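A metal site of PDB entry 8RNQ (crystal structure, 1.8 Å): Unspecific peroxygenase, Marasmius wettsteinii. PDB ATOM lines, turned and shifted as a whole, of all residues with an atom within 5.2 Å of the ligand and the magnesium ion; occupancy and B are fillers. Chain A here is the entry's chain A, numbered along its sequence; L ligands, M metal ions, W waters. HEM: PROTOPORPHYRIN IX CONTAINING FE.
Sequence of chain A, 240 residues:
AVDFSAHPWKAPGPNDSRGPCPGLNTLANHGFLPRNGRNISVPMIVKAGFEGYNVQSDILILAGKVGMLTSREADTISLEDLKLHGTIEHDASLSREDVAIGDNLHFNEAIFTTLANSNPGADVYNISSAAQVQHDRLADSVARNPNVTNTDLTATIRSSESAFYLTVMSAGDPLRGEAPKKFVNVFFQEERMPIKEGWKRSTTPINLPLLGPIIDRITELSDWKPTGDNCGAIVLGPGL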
ATOM      1  N   PRO A  20     -26.059  15.367  14.905  1.00  0.00           N
ATOM      2  CA  PRO A  20     -24.718  15.844  14.565  1.00  0.00           C
ATOM      3  C   PRO A  20     -23.824  14.856  13.831  1.00  0.00           C
ATOM      4  O   PRO A  20     -22.704  15.186  13.490  1.00  0.00           O
ATOM      5  CB  PRO A  20     -24.128  16.134  15.961  1.00  0.00           C
ATOM      6  CG  PRO A  20     -24.750  15.113  16.864  1.00  0.00           C
ATOM      7  CD  PRO A  20     -26.144  14.874  16.294  1.00  0.00           C
ATOM      8  N   CYS A  21     -24.354  13.642  13.607  1.00  0.00           N
ATOM      9  CA  CYS A  21     -23.574  12.545  13.043  1.00  0.00           C
ATOM     10  C   CYS A  21     -23.940  12.340  11.578  1.00  0.00           C
ATOM     11  O   CYS A  21     -25.032  11.876  11.278  1.00  0.00           O
ATOM     12  CB  CYS A  21     -23.793  11.258  13.789  1.00  0.00           C
ATOM     13  SG  CYS A  21     -22.955   9.838  13.029  1.00  0.00           S
ATOM     14  N   PRO A  22     -23.013  12.597  10.648  1.00  0.00           N
ATOM     15  CA  PRO A  22     -23.277  12.338   9.222  1.00  0.00           C
ATOM     16  C   PRO A  22     -23.440  10.850   8.900  1.00  0.00           C
ATOM     17  O   PRO A  22     -24.121  10.484   7.939  1.00  0.00           O
ATOM     18  CB  PRO A  22     -22.054  12.903   8.512  1.00  0.00           C
ATOM     19  CG  PRO A  22     -20.939  12.850   9.580  1.00  0.00           C
ATOM     20  CD  PRO A  22     -21.664  13.110  10.870  1.00  0.00           C
ATOM     21  N   GLY A  23     -22.849   9.979   9.731  1.00  0.00           N
ATOM     22  CA  GLY A  23     -22.953   8.557   9.467  1.00  0.00           C
ATOM     23  C   GLY A  23     -24.383   8.057   9.645  1.00  0.00           C
ATOM     24  O   GLY A  23     -24.940   7.340   8.816  1.00  0.00           O
ATOM     25  N   LEU A  24     -24.977   8.407  10.789  1.00  0.00           N
ATOM     26  CA  LEU A  24     -26.330   8.013  11.088  1.00  0.00           C
ATOM     27  C   LEU A  24     -27.322   8.803  10.219  1.00  0.00           C
ATOM     28  O   LEU A  24     -28.339   8.244   9.808  1.00  0.00           O
ATOM     29  CB  LEU A  24     -26.609   8.213  12.580  1.00  0.00           C
ATOM     30  CG  LEU A  24     -25.759   7.331  13.509  1.00  0.00           C
ATOM     31  CD1 LEU A  24     -26.141   7.578  14.940  1.00  0.00           C
ATOM     32  CD2 LEU A  24     -25.887   5.837  13.175  1.00  0.00           C
ATOM     33  N   LEU A  27     -27.504   7.130   6.824  1.00  0.00           N
ATOM     34  CA  LEU A  27     -28.272   5.903   6.864  1.00  0.00           C
ATOM     35  C   LEU A  27     -29.774   6.199   6.866  1.00  0.00           C
ATOM     36  O   LEU A  27     -30.548   5.521   6.179  1.00  0.00           O
ATOM     37  CB  LEU A  27     -27.825   5.073   8.077  1.00  0.00           C
ATOM     38  CG  LEU A  27     -26.429   4.468   7.991  1.00  0.00           C
ATOM     39  CD1 LEU A  27     -26.042   3.854   9.329  1.00  0.00           C
ATOM     40  CD2 LEU A  27     -26.343   3.416   6.898  1.00  0.00           C
ATOM     41  N   ILE A  45     -29.298   0.360  14.814  1.00  0.00           N
ATOM     42  CA  ILE A  45     -28.043   0.969  14.412  1.00  0.00           C
ATOM     43  C   ILE A  45     -27.050  -0.109  13.940  1.00  0.00           C
ATOM     44  O   ILE A  45     -26.357   0.075  12.946  1.00  0.00           O
ATOM     45  CB  ILE A  45     -27.460   1.831  15.561  1.00  0.00           C
ATOM     46  CG1 ILE A  45     -28.316   3.073  15.791  1.00  0.00           C
ATOM     47  CG2 ILE A  45     -26.046   2.201  15.252  1.00  0.00           C
ATOM     48  CD1 ILE A  45     -28.047   3.827  17.093  1.00  0.00           C
ATOM     49  N   TYR A  53     -22.707   0.143   5.441  1.00  0.00           N
ATOM     50  CA  TYR A  53     -21.312   0.542   5.420  1.00  0.00           C
ATOM     51  C   TYR A  53     -20.337  -0.622   5.671  1.00  0.00           C
ATOM     52  O   TYR A  53     -19.118  -0.429   5.505  1.00  0.00           O
ATOM     53  CB  TYR A  53     -21.022   1.574   6.534  1.00  0.00           C
ATOM     54  CG  TYR A  53     -21.779   2.879   6.507  1.00  0.00           C
ATOM     55  CD1 TYR A  53     -22.047   3.558   5.329  1.00  0.00           C
ATOM     56  CD2 TYR A  53     -22.161   3.498   7.682  1.00  0.00           C
ATOM     57  CE1 TYR A  53     -22.705   4.770   5.319  1.00  0.00           C
ATOM     58  CE2 TYR A  53     -22.845   4.707   7.695  1.00  0.00           C
ATOM     59  CZ  TYR A  53     -23.078   5.380   6.506  1.00  0.00           C
ATOM     60  OH  TYR A  53     -23.753   6.582   6.474  1.00  0.00           O
ATOM     61  N   VAL A  55     -19.887  -1.682   8.624  1.00  0.00           N
ATOM     62  CA  VAL A  55     -19.343  -1.463   9.968  1.00  0.00           C
ATOM     63  C   VAL A  55     -19.918  -2.507  10.914  1.00  0.00           C
ATOM     64  O   VAL A  55     -21.101  -2.790  10.915  1.00  0.00           O
ATOM     65  CB  VAL A  55     -19.595  -0.023  10.441  1.00  0.00           C
ATOM     66  CG1 VAL A  55     -19.170   0.170  11.891  1.00  0.00           C
ATOM     67  CG2 VAL A  55     -18.925   0.993   9.568  1.00  0.00           C
ATOM     68  N   ILE A  59     -18.006  -1.833  17.341  1.00  0.00           N
ATOM     69  CA  ILE A  59     -17.938  -0.378  17.564  1.00  0.00           C
ATOM     70  C   ILE A  59     -19.345   0.204  17.697  1.00  0.00           C
ATOM     71  O   ILE A  59     -19.554   1.169  18.438  1.00  0.00           O
ATOM     72  CB  ILE A  59     -17.108   0.341  16.484  1.00  0.00           C
ATOM     73  CG1 ILE A  59     -16.989   1.823  16.831  1.00  0.00           C
ATOM     74  CG2 ILE A  59     -17.692   0.105  15.112  1.00  0.00           C
ATOM     75  CD1 ILE A  59     -15.946   2.584  16.064  1.00  0.00           C
ATOM     76  N   LEU A  60     -20.339  -0.364  16.986  1.00  0.00           N
ATOM     77  CA  LEU A  60     -21.692   0.180  16.984  1.00  0.00           C
ATOM     78  C   LEU A  60     -22.434  -0.114  18.274  1.00  0.00           C
ATOM     79  O   LEU A  60     -23.237   0.725  18.690  1.00  0.00           O
ATOM     80  CB  LEU A  60     -22.458  -0.332  15.765  1.00  0.00           C
ATOM     81  CG  LEU A  60     -21.901   0.151  14.427  1.00  0.00           C
ATOM     82  CD1 LEU A  60     -22.692  -0.413  13.265  1.00  0.00           C
ATOM     83  CD2 LEU A  60     -21.883   1.690  14.324  1.00  0.00           C
ATOM     84  N   ALA A  63     -20.560   2.447  20.898  1.00  0.00           N
ATOM     85  CA  ALA A  63     -20.998   3.828  20.647  1.00  0.00           C
ATOM     86  C   ALA A  63     -22.506   3.989  20.826  1.00  0.00           C
ATOM     87  O   ALA A  63     -22.962   4.968  21.389  1.00  0.00           O
ATOM     88  CB  ALA A  63     -20.603   4.275  19.251  1.00  0.00           C
ATOM     89  N   GLY A  64     -23.275   3.001  20.333  1.00  0.00           N
ATOM     90  CA  GLY A  64     -24.725   3.056  20.379  1.00  0.00           C
ATOM     91  C   GLY A  64     -25.259   3.165  21.805  1.00  0.00           C
ATOM     92  O   GLY A  64     -26.189   3.923  22.087  1.00  0.00           O
ATOM     93  N   GLY A  67     -24.714   6.472  23.142  1.00  0.00           N
ATOM     94  CA  GLY A  67     -25.684   7.365  22.536  1.00  0.00           C
ATOM     95  C   GLY A  67     -27.083   7.259  23.146  1.00  0.00           C
ATOM     96  O   GLY A  67     -27.810   8.236  23.206  1.00  0.00           O
ATOM     97  N   LEU A  82     -28.744  13.112  19.943  1.00  0.00           N
ATOM     98  CA  LEU A  82     -27.306  12.902  20.021  1.00  0.00           C
ATOM     99  C   LEU A  82     -26.520  14.225  20.098  1.00  0.00           C
ATOM    100  O   LEU A  82     -25.302  14.207  20.304  1.00  0.00           O
ATOM    101  CB  LEU A  82     -26.851  12.097  18.804  1.00  0.00           C
ATOM    102  CG  LEU A  82     -27.327  10.647  18.770  1.00  0.00           C
ATOM    103  CD1 LEU A  82     -26.939   9.999  17.465  1.00  0.00           C
ATOM    104  CD2 LEU A  82     -26.786   9.843  19.950  1.00  0.00           C
ATOM    105  N   ILE A  88     -21.482  12.227  23.767  1.00  0.00           N
ATOM    106  CA  ILE A  88     -20.545  12.052  22.676  1.00  0.00           C
ATOM    107  C   ILE A  88     -20.195  13.406  22.025  1.00  0.00           C
ATOM    108  O   ILE A  88     -19.043  13.667  21.690  1.00  0.00           O
ATOM    109  CB  ILE A  88     -21.104  11.058  21.637  1.00  0.00           C
ATOM    110  CG1 ILE A  88     -21.235   9.635  22.212  1.00  0.00           C
ATOM    111  CG2 ILE A  88     -20.238  11.039  20.393  1.00  0.00           C
ATOM    112  CD1 ILE A  88     -21.981   8.669  21.310  1.00  0.00           C
ATOM    113  N   GLU A  89     -21.199  14.260  21.805  1.00  0.00           N
ATOM    114  CA  GLU A  89     -21.005  15.519  21.077  1.00  0.00           C
ATOM    115  C   GLU A  89     -19.942  16.373  21.779  1.00  0.00           C
ATOM    116  O   GLU A  89     -19.928  16.472  23.002  1.00  0.00           O
ATOM    117  CB  GLU A  89     -22.329  16.259  20.908  1.00  0.00           C
ATOM    118  CG  GLU A  89     -22.259  17.385  19.892  1.00  0.00           C
ATOM    119  CD  GLU A  89     -21.554  18.647  20.377  1.00  0.00           C
ATOM    120  OE1 GLU A  89     -21.791  18.989  21.538  1.00  0.00           O
ATOM    121  OE2 GLU A  89     -20.796  19.240  19.576  1.00  0.00           O
ATOM    122  N   HIS A  90     -19.010  16.889  20.983  1.00  0.00           N
ATOM    123  CA  HIS A  90     -17.824  17.547  21.500  1.00  0.00           C
ATOM    124  C   HIS A  90     -17.528  18.795  20.696  1.00  0.00           C
ATOM    125  O   HIS A  90     -17.918  18.971  19.536  1.00  0.00           O
ATOM    126  CB  HIS A  90     -16.629  16.568  21.448  1.00  0.00           C
ATOM    127  CG  HIS A  90     -16.412  16.043  20.074  1.00  0.00           C
ATOM    128  ND1 HIS A  90     -15.916  16.771  19.011  1.00  0.00           N
ATOM    129  CD2 HIS A  90     -16.742  14.810  19.576  1.00  0.00           C
ATOM    130  CE1 HIS A  90     -15.974  16.030  17.916  1.00  0.00           C
ATOM    131  NE2 HIS A  90     -16.470  14.826  18.233  1.00  0.00           N
ATOM    132  N   ASP A  91     -16.674  19.658  21.273  1.00  0.00           N
ATOM    133  CA  ASP A  91     -16.094  20.775  20.536  1.00  0.00           C
ATOM    134  C   ASP A  91     -15.088  20.307  19.484  1.00  0.00           C
ATOM    135  O   ASP A  91     -14.630  19.156  19.517  1.00  0.00           O
ATOM    136  CB  ASP A  91     -15.404  21.721  21.533  1.00  0.00           C
ATOM    137  CG  ASP A  91     -16.337  22.266  22.599  1.00  0.00           C
ATOM    138  OD1 ASP A  91     -17.520  22.459  22.271  1.00  0.00           O
ATOM    139  OD2 ASP A  91     -15.860  22.535  23.741  1.00  0.00           O
ATOM    140  N   SER A  93     -15.499  19.899  16.310  1.00  0.00           N
ATOM    141  CA  SER A  93     -16.082  19.083  15.249  1.00  0.00           C
ATOM    142  C   SER A  93     -15.554  19.507  13.880  1.00  0.00           C
ATOM    143  O   SER A  93     -15.035  20.589  13.683  1.00  0.00           O
ATOM    144  CB  SER A  93     -17.602  19.183  15.302  1.00  0.00           C
ATOM    145  OG  SER A  93     -18.149  18.578  16.457  1.00  0.00           O
ATOM    146  N   LEU A  94     -15.675  18.590  12.917  1.00  0.00           N
ATOM    147  CA  LEU A  94     -15.173  18.816  11.579  1.00  0.00           C
ATOM    148  C   LEU A  94     -16.141  19.663  10.734  1.00  0.00           C
ATOM    149  O   LEU A  94     -15.733  20.148   9.705  1.00  0.00           O
ATOM    150  CB  LEU A  94     -14.989  17.439  10.900  1.00  0.00           C
ATOM    151  CG  LEU A  94     -13.983  16.462  11.530  1.00  0.00           C
ATOM    152  CD1 LEU A  94     -14.190  15.021  10.989  1.00  0.00           C
ATOM    153  CD2 LEU A  94     -12.569  16.929  11.326  1.00  0.00           C
ATOM    154  N   SER A  95     -17.431  19.662  11.072  1.00  0.00           N
ATOM    155  CA  SER A  95     -18.470  20.177  10.192  1.00  0.00           C
ATOM    156  C   SER A  95     -19.571  20.926  10.958  1.00  0.00           C
ATOM    157  O   SER A  95     -20.543  21.375  10.341  1.00  0.00           O
ATOM    158  CB  SER A  95     -19.043  19.057   9.318  1.00  0.00           C
ATOM    159  OG  SER A  95     -19.916  18.237  10.058  1.00  0.00           O
ATOM    160  N   ARG A  96     -19.464  20.996  12.297  1.00  0.00           N
ATOM    161  CA  ARG A  96     -20.409  21.666  13.164  1.00  0.00           C
ATOM    162  C   ARG A  96     -19.654  22.680  14.024  1.00  0.00           C
ATOM    163  O   ARG A  96     -18.455  22.533  14.236  1.00  0.00           O
ATOM    164  CB  ARG A  96     -21.128  20.690  14.085  1.00  0.00           C
ATOM    165  CG  ARG A  96     -22.408  20.065  13.533  1.00  0.00           C
ATOM    166  CD  ARG A  96     -22.220  19.233  12.284  1.00  0.00           C
ATOM    167  NE  ARG A  96     -23.395  18.435  12.015  1.00  0.00           N
ATOM    168  CZ  ARG A  96     -23.577  17.737  10.904  1.00  0.00           C
ATOM    169  NH1 ARG A  96     -22.600  17.629  10.010  1.00  0.00           N
ATOM    170  NH2 ARG A  96     -24.749  17.131  10.707  1.00  0.00           N
ATOM    171  N   GLU A  97     -20.389  23.643  14.573  1.00  0.00           N
ATOM    172  CA  GLU A  97     -19.782  24.673  15.434  1.00  0.00           C
ATOM    173  C   GLU A  97     -19.818  24.183  16.877  1.00  0.00           C
ATOM    174  O   GLU A  97     -20.615  23.301  17.230  1.00  0.00           O
ATOM    175  CB  GLU A  97     -20.570  25.988  15.318  1.00  0.00           C
ATOM    176  CG  GLU A  97     -20.544  26.582  13.917  1.00  0.00           C
ATOM    177  CD  GLU A  97     -21.444  27.807  13.700  1.00  0.00           C
ATOM    178  OE1 GLU A  97     -22.454  27.939  14.393  1.00  0.00           O
ATOM    179  OE2 GLU A  97     -21.076  28.660  12.860  1.00  0.00           O
ATOM    180  N   ASN A 104     -24.345  23.273  17.217  1.00  0.00           N
ATOM    181  CA  ASN A 104     -23.551  22.064  17.375  1.00  0.00           C
ATOM    182  C   ASN A 104     -24.237  20.900  16.640  1.00  0.00           C
ATOM    183  O   ASN A 104     -23.780  19.761  16.776  1.00  0.00           O
ATOM    184  CB  ASN A 104     -23.303  21.691  18.836  1.00  0.00           C
ATOM    185  CG  ASN A 104     -24.511  21.159  19.573  1.00  0.00           C
ATOM    186  OD1 ASN A 104     -25.654  21.366  19.179  1.00  0.00           O
ATOM    187  ND2 ASN A 104     -24.269  20.453  20.661  1.00  0.00           N
ATOM    188  N   GLU A 161     -13.868   9.434  14.651  1.00  0.00           N
ATOM    189  CA  GLU A 161     -14.738  10.025  13.655  1.00  0.00           C
ATOM    190  C   GLU A 161     -13.986  10.245  12.365  1.00  0.00           C
ATOM    191  O   GLU A 161     -14.549  10.035  11.278  1.00  0.00           O
ATOM    192  CB  GLU A 161     -15.397  11.283  14.238  1.00  0.00           C
ATOM    193  CG  GLU A 161     -16.427  10.938  15.305  1.00  0.00           C
ATOM    194  CD  GLU A 161     -16.844  11.993  16.334  1.00  0.00           C
ATOM    195  OE1 GLU A 161     -16.352  13.093  16.287  1.00  0.00           O
ATOM    196  OE2 GLU A 161     -17.754  11.674  17.142  1.00  0.00           O
ATOM    197  N   PHE A 164     -13.557   7.001  10.722  1.00  0.00           N
ATOM    198  CA  PHE A 164     -14.807   6.615  10.104  1.00  0.00           C
ATOM    199  C   PHE A 164     -14.916   7.200   8.692  1.00  0.00           C
ATOM    200  O   PHE A 164     -15.198   6.463   7.748  1.00  0.00           O
ATOM    201  CB  PHE A 164     -16.009   7.000  10.954  1.00  0.00           C
ATOM    202  CG  PHE A 164     -16.554   5.927  11.849  1.00  0.00           C
ATOM    203  CD1 PHE A 164     -16.619   4.606  11.398  1.00  0.00           C
ATOM    204  CD2 PHE A 164     -17.188   6.243  13.041  1.00  0.00           C
ATOM    205  CE1 PHE A 164     -17.175   3.608  12.184  1.00  0.00           C
ATOM    206  CE2 PHE A 164     -17.756   5.249  13.822  1.00  0.00           C
ATOM    207  CZ  PHE A 164     -17.756   3.928  13.386  1.00  0.00           C
ATOM    208  N   TYR A 165     -14.699   8.514   8.507  1.00  0.00           N
ATOM    209  CA  TYR A 165     -14.903   9.011   7.146  1.00  0.00           C
ATOM    210  C   TYR A 165     -13.851   8.462   6.191  1.00  0.00           C
ATOM    211  O   TYR A 165     -14.184   8.193   5.029  1.00  0.00           O
ATOM    212  CB  TYR A 165     -15.055  10.533   7.091  1.00  0.00           C
ATOM    213  CG  TYR A 165     -13.819  11.374   7.196  1.00  0.00           C
ATOM    214  CD1 TYR A 165     -12.886  11.409   6.188  1.00  0.00           C
ATOM    215  CD2 TYR A 165     -13.636  12.188   8.293  1.00  0.00           C
ATOM    216  CE1 TYR A 165     -11.756  12.199   6.279  1.00  0.00           C
ATOM    217  CE2 TYR A 165     -12.522  12.981   8.422  1.00  0.00           C
ATOM    218  CZ  TYR A 165     -11.573  12.988   7.414  1.00  0.00           C
ATOM    219  OH  TYR A 165     -10.466  13.805   7.483  1.00  0.00           O
ATOM    220  N   VAL A 168     -15.253   4.408   5.736  1.00  0.00           N
ATOM    221  CA  VAL A 168     -16.581   4.055   5.246  1.00  0.00           C
ATOM    222  C   VAL A 168     -16.767   4.601   3.820  1.00  0.00           C
ATOM    223  O   VAL A 168     -17.463   4.007   2.990  1.00  0.00           O
ATOM    224  CB  VAL A 168     -17.636   4.561   6.251  1.00  0.00           C
ATOM    225  CG1 VAL A 168     -19.018   4.627   5.664  1.00  0.00           C
ATOM    226  CG2 VAL A 168     -17.657   3.728   7.527  1.00  0.00           C
ATOM    227  N   PHE A 187     -20.688  12.919   1.388  1.00  0.00           N
ATOM    228  CA  PHE A 187     -21.092  12.356   2.669  1.00  0.00           C
ATOM    229  C   PHE A 187     -21.425  13.465   3.686  1.00  0.00           C
ATOM    230  O   PHE A 187     -22.503  13.457   4.308  1.00  0.00           O
ATOM    231  CB  PHE A 187     -19.973  11.405   3.128  1.00  0.00           C
ATOM    232  CG  PHE A 187     -20.185  10.780   4.474  1.00  0.00           C
ATOM    233  CD1 PHE A 187     -21.169   9.832   4.694  1.00  0.00           C
ATOM    234  CD2 PHE A 187     -19.340  11.093   5.519  1.00  0.00           C
ATOM    235  CE1 PHE A 187     -21.326   9.227   5.945  1.00  0.00           C
ATOM    236  CE2 PHE A 187     -19.501  10.515   6.761  1.00  0.00           C
ATOM    237  CZ  PHE A 187     -20.486   9.569   6.967  1.00  0.00           C
ATOM    238  N   PHE A 188     -20.526  14.430   3.881  1.00  0.00           N
ATOM    239  CA  PHE A 188     -20.724  15.511   4.845  1.00  0.00           C
ATOM    240  C   PHE A 188     -21.746  16.546   4.351  1.00  0.00           C
ATOM    241  O   PHE A 188     -22.650  16.937   5.111  1.00  0.00           O
ATOM    242  CB  PHE A 188     -19.389  16.205   5.117  1.00  0.00           C
ATOM    243  CG  PHE A 188     -18.497  15.552   6.164  1.00  0.00           C
ATOM    244  CD1 PHE A 188     -18.655  15.833   7.509  1.00  0.00           C
ATOM    245  CD2 PHE A 188     -17.498  14.670   5.802  1.00  0.00           C
ATOM    246  CE1 PHE A 188     -17.815  15.257   8.453  1.00  0.00           C
ATOM    247  CE2 PHE A 188     -16.654  14.111   6.748  1.00  0.00           C
ATOM    248  CZ  PHE A 188     -16.815  14.408   8.075  1.00  0.00           C
HETATM  249  CHA HEM L   1     -20.020  12.484  14.737  1.00  0.00           C
HETATM  250  CHB HEM L   1     -22.713   9.511  17.279  1.00  0.00           C
HETATM  251  CHC HEM L   1     -21.861   5.999  14.061  1.00  0.00           C
HETATM  252  CHD HEM L   1     -19.315   9.110  11.435  1.00  0.00           C
HETATM  253  C1A HEM L   1     -20.847  11.979  15.648  1.00  0.00           C
HETATM  254  C2A HEM L   1     -21.339  12.746  16.774  1.00  0.00           C
HETATM  255  C3A HEM L   1     -22.141  11.935  17.466  1.00  0.00           C
HETATM  256  C4A HEM L   1     -22.075  10.634  16.819  1.00  0.00           C
HETATM  257  CMA HEM L   1     -22.916  12.246  18.706  1.00  0.00           C
HETATM  258  CAA HEM L   1     -21.088  14.222  16.978  1.00  0.00           C
HETATM  259  CBA HEM L   1     -19.639  14.374  17.492  1.00  0.00           C
HETATM  260  CGA HEM L   1     -19.236  15.811  17.277  1.00  0.00           C
HETATM  261  O1A HEM L   1     -19.388  16.669  18.145  1.00  0.00           O
HETATM  262  O2A HEM L   1     -18.759  16.138  16.198  1.00  0.00           O
HETATM  263  C1B HEM L   1     -22.674   8.250  16.649  1.00  0.00           C
HETATM  264  C2B HEM L   1     -23.287   7.113  17.191  1.00  0.00           C
HETATM  265  C3B HEM L   1     -23.055   6.107  16.274  1.00  0.00           C
HETATM  266  C4B HEM L   1     -22.242   6.694  15.214  1.00  0.00           C
HETATM  267  CMB HEM L   1     -24.104   6.972  18.429  1.00  0.00           C
HETATM  268  CAB HEM L   1     -23.375   4.665  16.328  1.00  0.00           C
HETATM  269  CBB HEM L   1     -23.501   3.968  17.408  1.00  0.00           C
HETATM  270  C1C HEM L   1     -21.225   6.551  12.995  1.00  0.00           C
HETATM  271  C2C HEM L   1     -20.943   5.899  11.751  1.00  0.00           C
HETATM  272  C3C HEM L   1     -20.182   6.748  11.033  1.00  0.00           C
HETATM  273  C4C HEM L   1     -20.011   7.987  11.792  1.00  0.00           C
HETATM  274  CMC HEM L   1     -21.460   4.463  11.470  1.00  0.00           C
HETATM  275  CAC HEM L   1     -19.739   6.425   9.684  1.00  0.00           C
HETATM  276  CBC HEM L   1     -18.870   7.086   9.008  1.00  0.00           C
HETATM  277  C1D HEM L   1     -19.264  10.317  12.155  1.00  0.00           C
HETATM  278  C2D HEM L   1     -18.414  11.451  11.765  1.00  0.00           C
HETATM  279  C3D HEM L   1     -18.632  12.408  12.707  1.00  0.00           C
HETATM  280  C4D HEM L   1     -19.549  11.789  13.633  1.00  0.00           C
HETATM  281  CMD HEM L   1     -17.553  11.574  10.541  1.00  0.00           C
HETATM  282  CAD HEM L   1     -17.955  13.774  12.716  1.00  0.00           C
HETATM  283  CBD HEM L   1     -18.877  14.957  12.427  1.00  0.00           C
HETATM  284  CGD HEM L   1     -18.089  16.247  12.628  1.00  0.00           C
HETATM  285  O1D HEM L   1     -16.965  16.245  13.228  1.00  0.00           O
HETATM  286  O2D HEM L   1     -18.541  17.293  12.135  1.00  0.00           O
HETATM  287  NA  HEM L   1     -21.281  10.713  15.738  1.00  0.00           N
HETATM  288  NB  HEM L   1     -22.025   8.001  15.469  1.00  0.00           N
HETATM  289  NC  HEM L   1     -20.661   7.773  12.943  1.00  0.00           N
HETATM  290  ND  HEM L   1     -19.917  10.496  13.330  1.00  0.00           N
HETATM  291 FE   HEM L   1     -21.042   9.333  14.281  1.00  0.00          FE
HETATM  292 MG    MG M   1     -19.502  18.849  17.986  1.00  0.00          MG
HETATM  293  O   HOH W   1     -19.245  20.949  17.635  1.00  0.00           O
HETATM  294  O   HOH W   2     -15.171  15.095  14.875  1.00  0.00           O
HETATM  295  O   HOH W   3     -20.927  17.111  14.552  1.00  0.00           O
HETATM  296  O   HOH W   4     -21.239  18.619  16.827  1.00  0.00           O
HETATM  297  O   HOH W   5     -19.255   8.801  15.510  1.00  0.00           O
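Water W2 bridges O1D of the ligand and OE1 of Glu 161.
Water W3 lies within hydrogen-bond range of the backbone carbonyl oxygen (O) of Pro 20 (2.8 Å) and an oxygen (O2A) of the ligand (2.9 Å).
Residues that only touch the ligand: Gly 64 (3.1 Å), Glu 161 (3.3 Å), Ile 88 (3.4 Å), Ala 63 (3.4 Å), Phe 164 (3.5 Å), Leu 82 (3.5 Å), Leu 60 (3.5 Å), Phe 187 (3.6 Å), Pro 22 (3.6 Å), Gly 23 (3.7 Å), Leu 24 (3.7 Å), Pro 20 (3.7 Å), Ile 45 (3.8 Å), Arg 96 (3.8 Å), Phe 188 (3.8 Å), Val 168 (3.9 Å) and Tyr 53 (3.97 Å).
Hydrophobic or aromatic side chains within 4 Å of the ligand: Pro 20, Pro 22, Leu 24, Ile 45, Tyr 53, Leu 60, Ala 63, Leu 82, Ile 88, His 90, Leu 94, Phe 164, Val 168, Phe 187 and Phe 188.
Within 4 Å of the ligand: Pro 20, Cys 21, Pro 22, Gly 23, Leu 24, Ile 45, Tyr 53, Leu 60, Ala 63, Gly 64, Leu 82, Ile 88, Glu 89, His 90, Ser 93, Leu 94, Ser 95, Arg 96, Glu 161, Phe 164, Val 168, Phe 187 and Phe 188.
The nearest printed residue that does not touch the ligand is Tyr 165 (4.4 Å).
The magnesium ion is bound by the side-chain hydroxyl of Ser 93 (2.1 Å), the side-chain carboxylate of Glu 89 (2.1 Å), water W4 (2.1 Å), water W1 (2.1 Å), an oxygen (O1A) of the ligand (2.2 Å) and the backbone carbonyl oxygen of His 90 (2.2 Å).
SG of Cys 21 is bound to FE of the ligand, at 2.3 Å.
An oxygen (O2D) of the ligand is in hydrogen-bond range of the backbone NH (N) of Ser 95, at 2.8 Å.
An oxygen (O1A) of the ligand lies close to the backbone NH of His 90.
An oxygen (O2A) of the ligand lies close to a ring nitrogen (NE2) of His 90 (3.3 Å).
The backbone NH (N) of Leu 94 sits at hydrogen-bond distance from an oxygen (O1D) of the ligand (2.7 Å).
An oxygen (O2D) of the ligand lies within hydrogen-bond range of the side-chain hydroxyl (OG) of Ser 95 (2.7 Å).
The backbone NH of Gly 23 sits close to the side-chain sulfur of Cys 21, 3.3 Å away.
NH1 of Arg 96 is in hydrogen-bond range of OG of Ser 95, at 2.8 Å.
The side-chain hydroxyl of Tyr 53 sits at hydrogen-bond distance from the backbone carbonyl oxygen of Gly 23, 2.7 Å away.
OE1 of Glu 161 sits at hydrogen-bond distance from NE2 of His 90.
The side-chain carboxylate of Glu 89 lies within hydrogen-bond range of the side-chain amide nitrogen of Asn 104, at 3.0 Å.
The backbone NH (N) of Leu 24 lies close to the side-chain sulfur (SG) of Cys 21 (3.3 Å).
Three residues have an atom within 4 Å of the magnesium ion: Glu 89, His 90 and Ser 93.
Along chain A the residues within 4 Å of the magnesium ion span positions 89 to 93.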
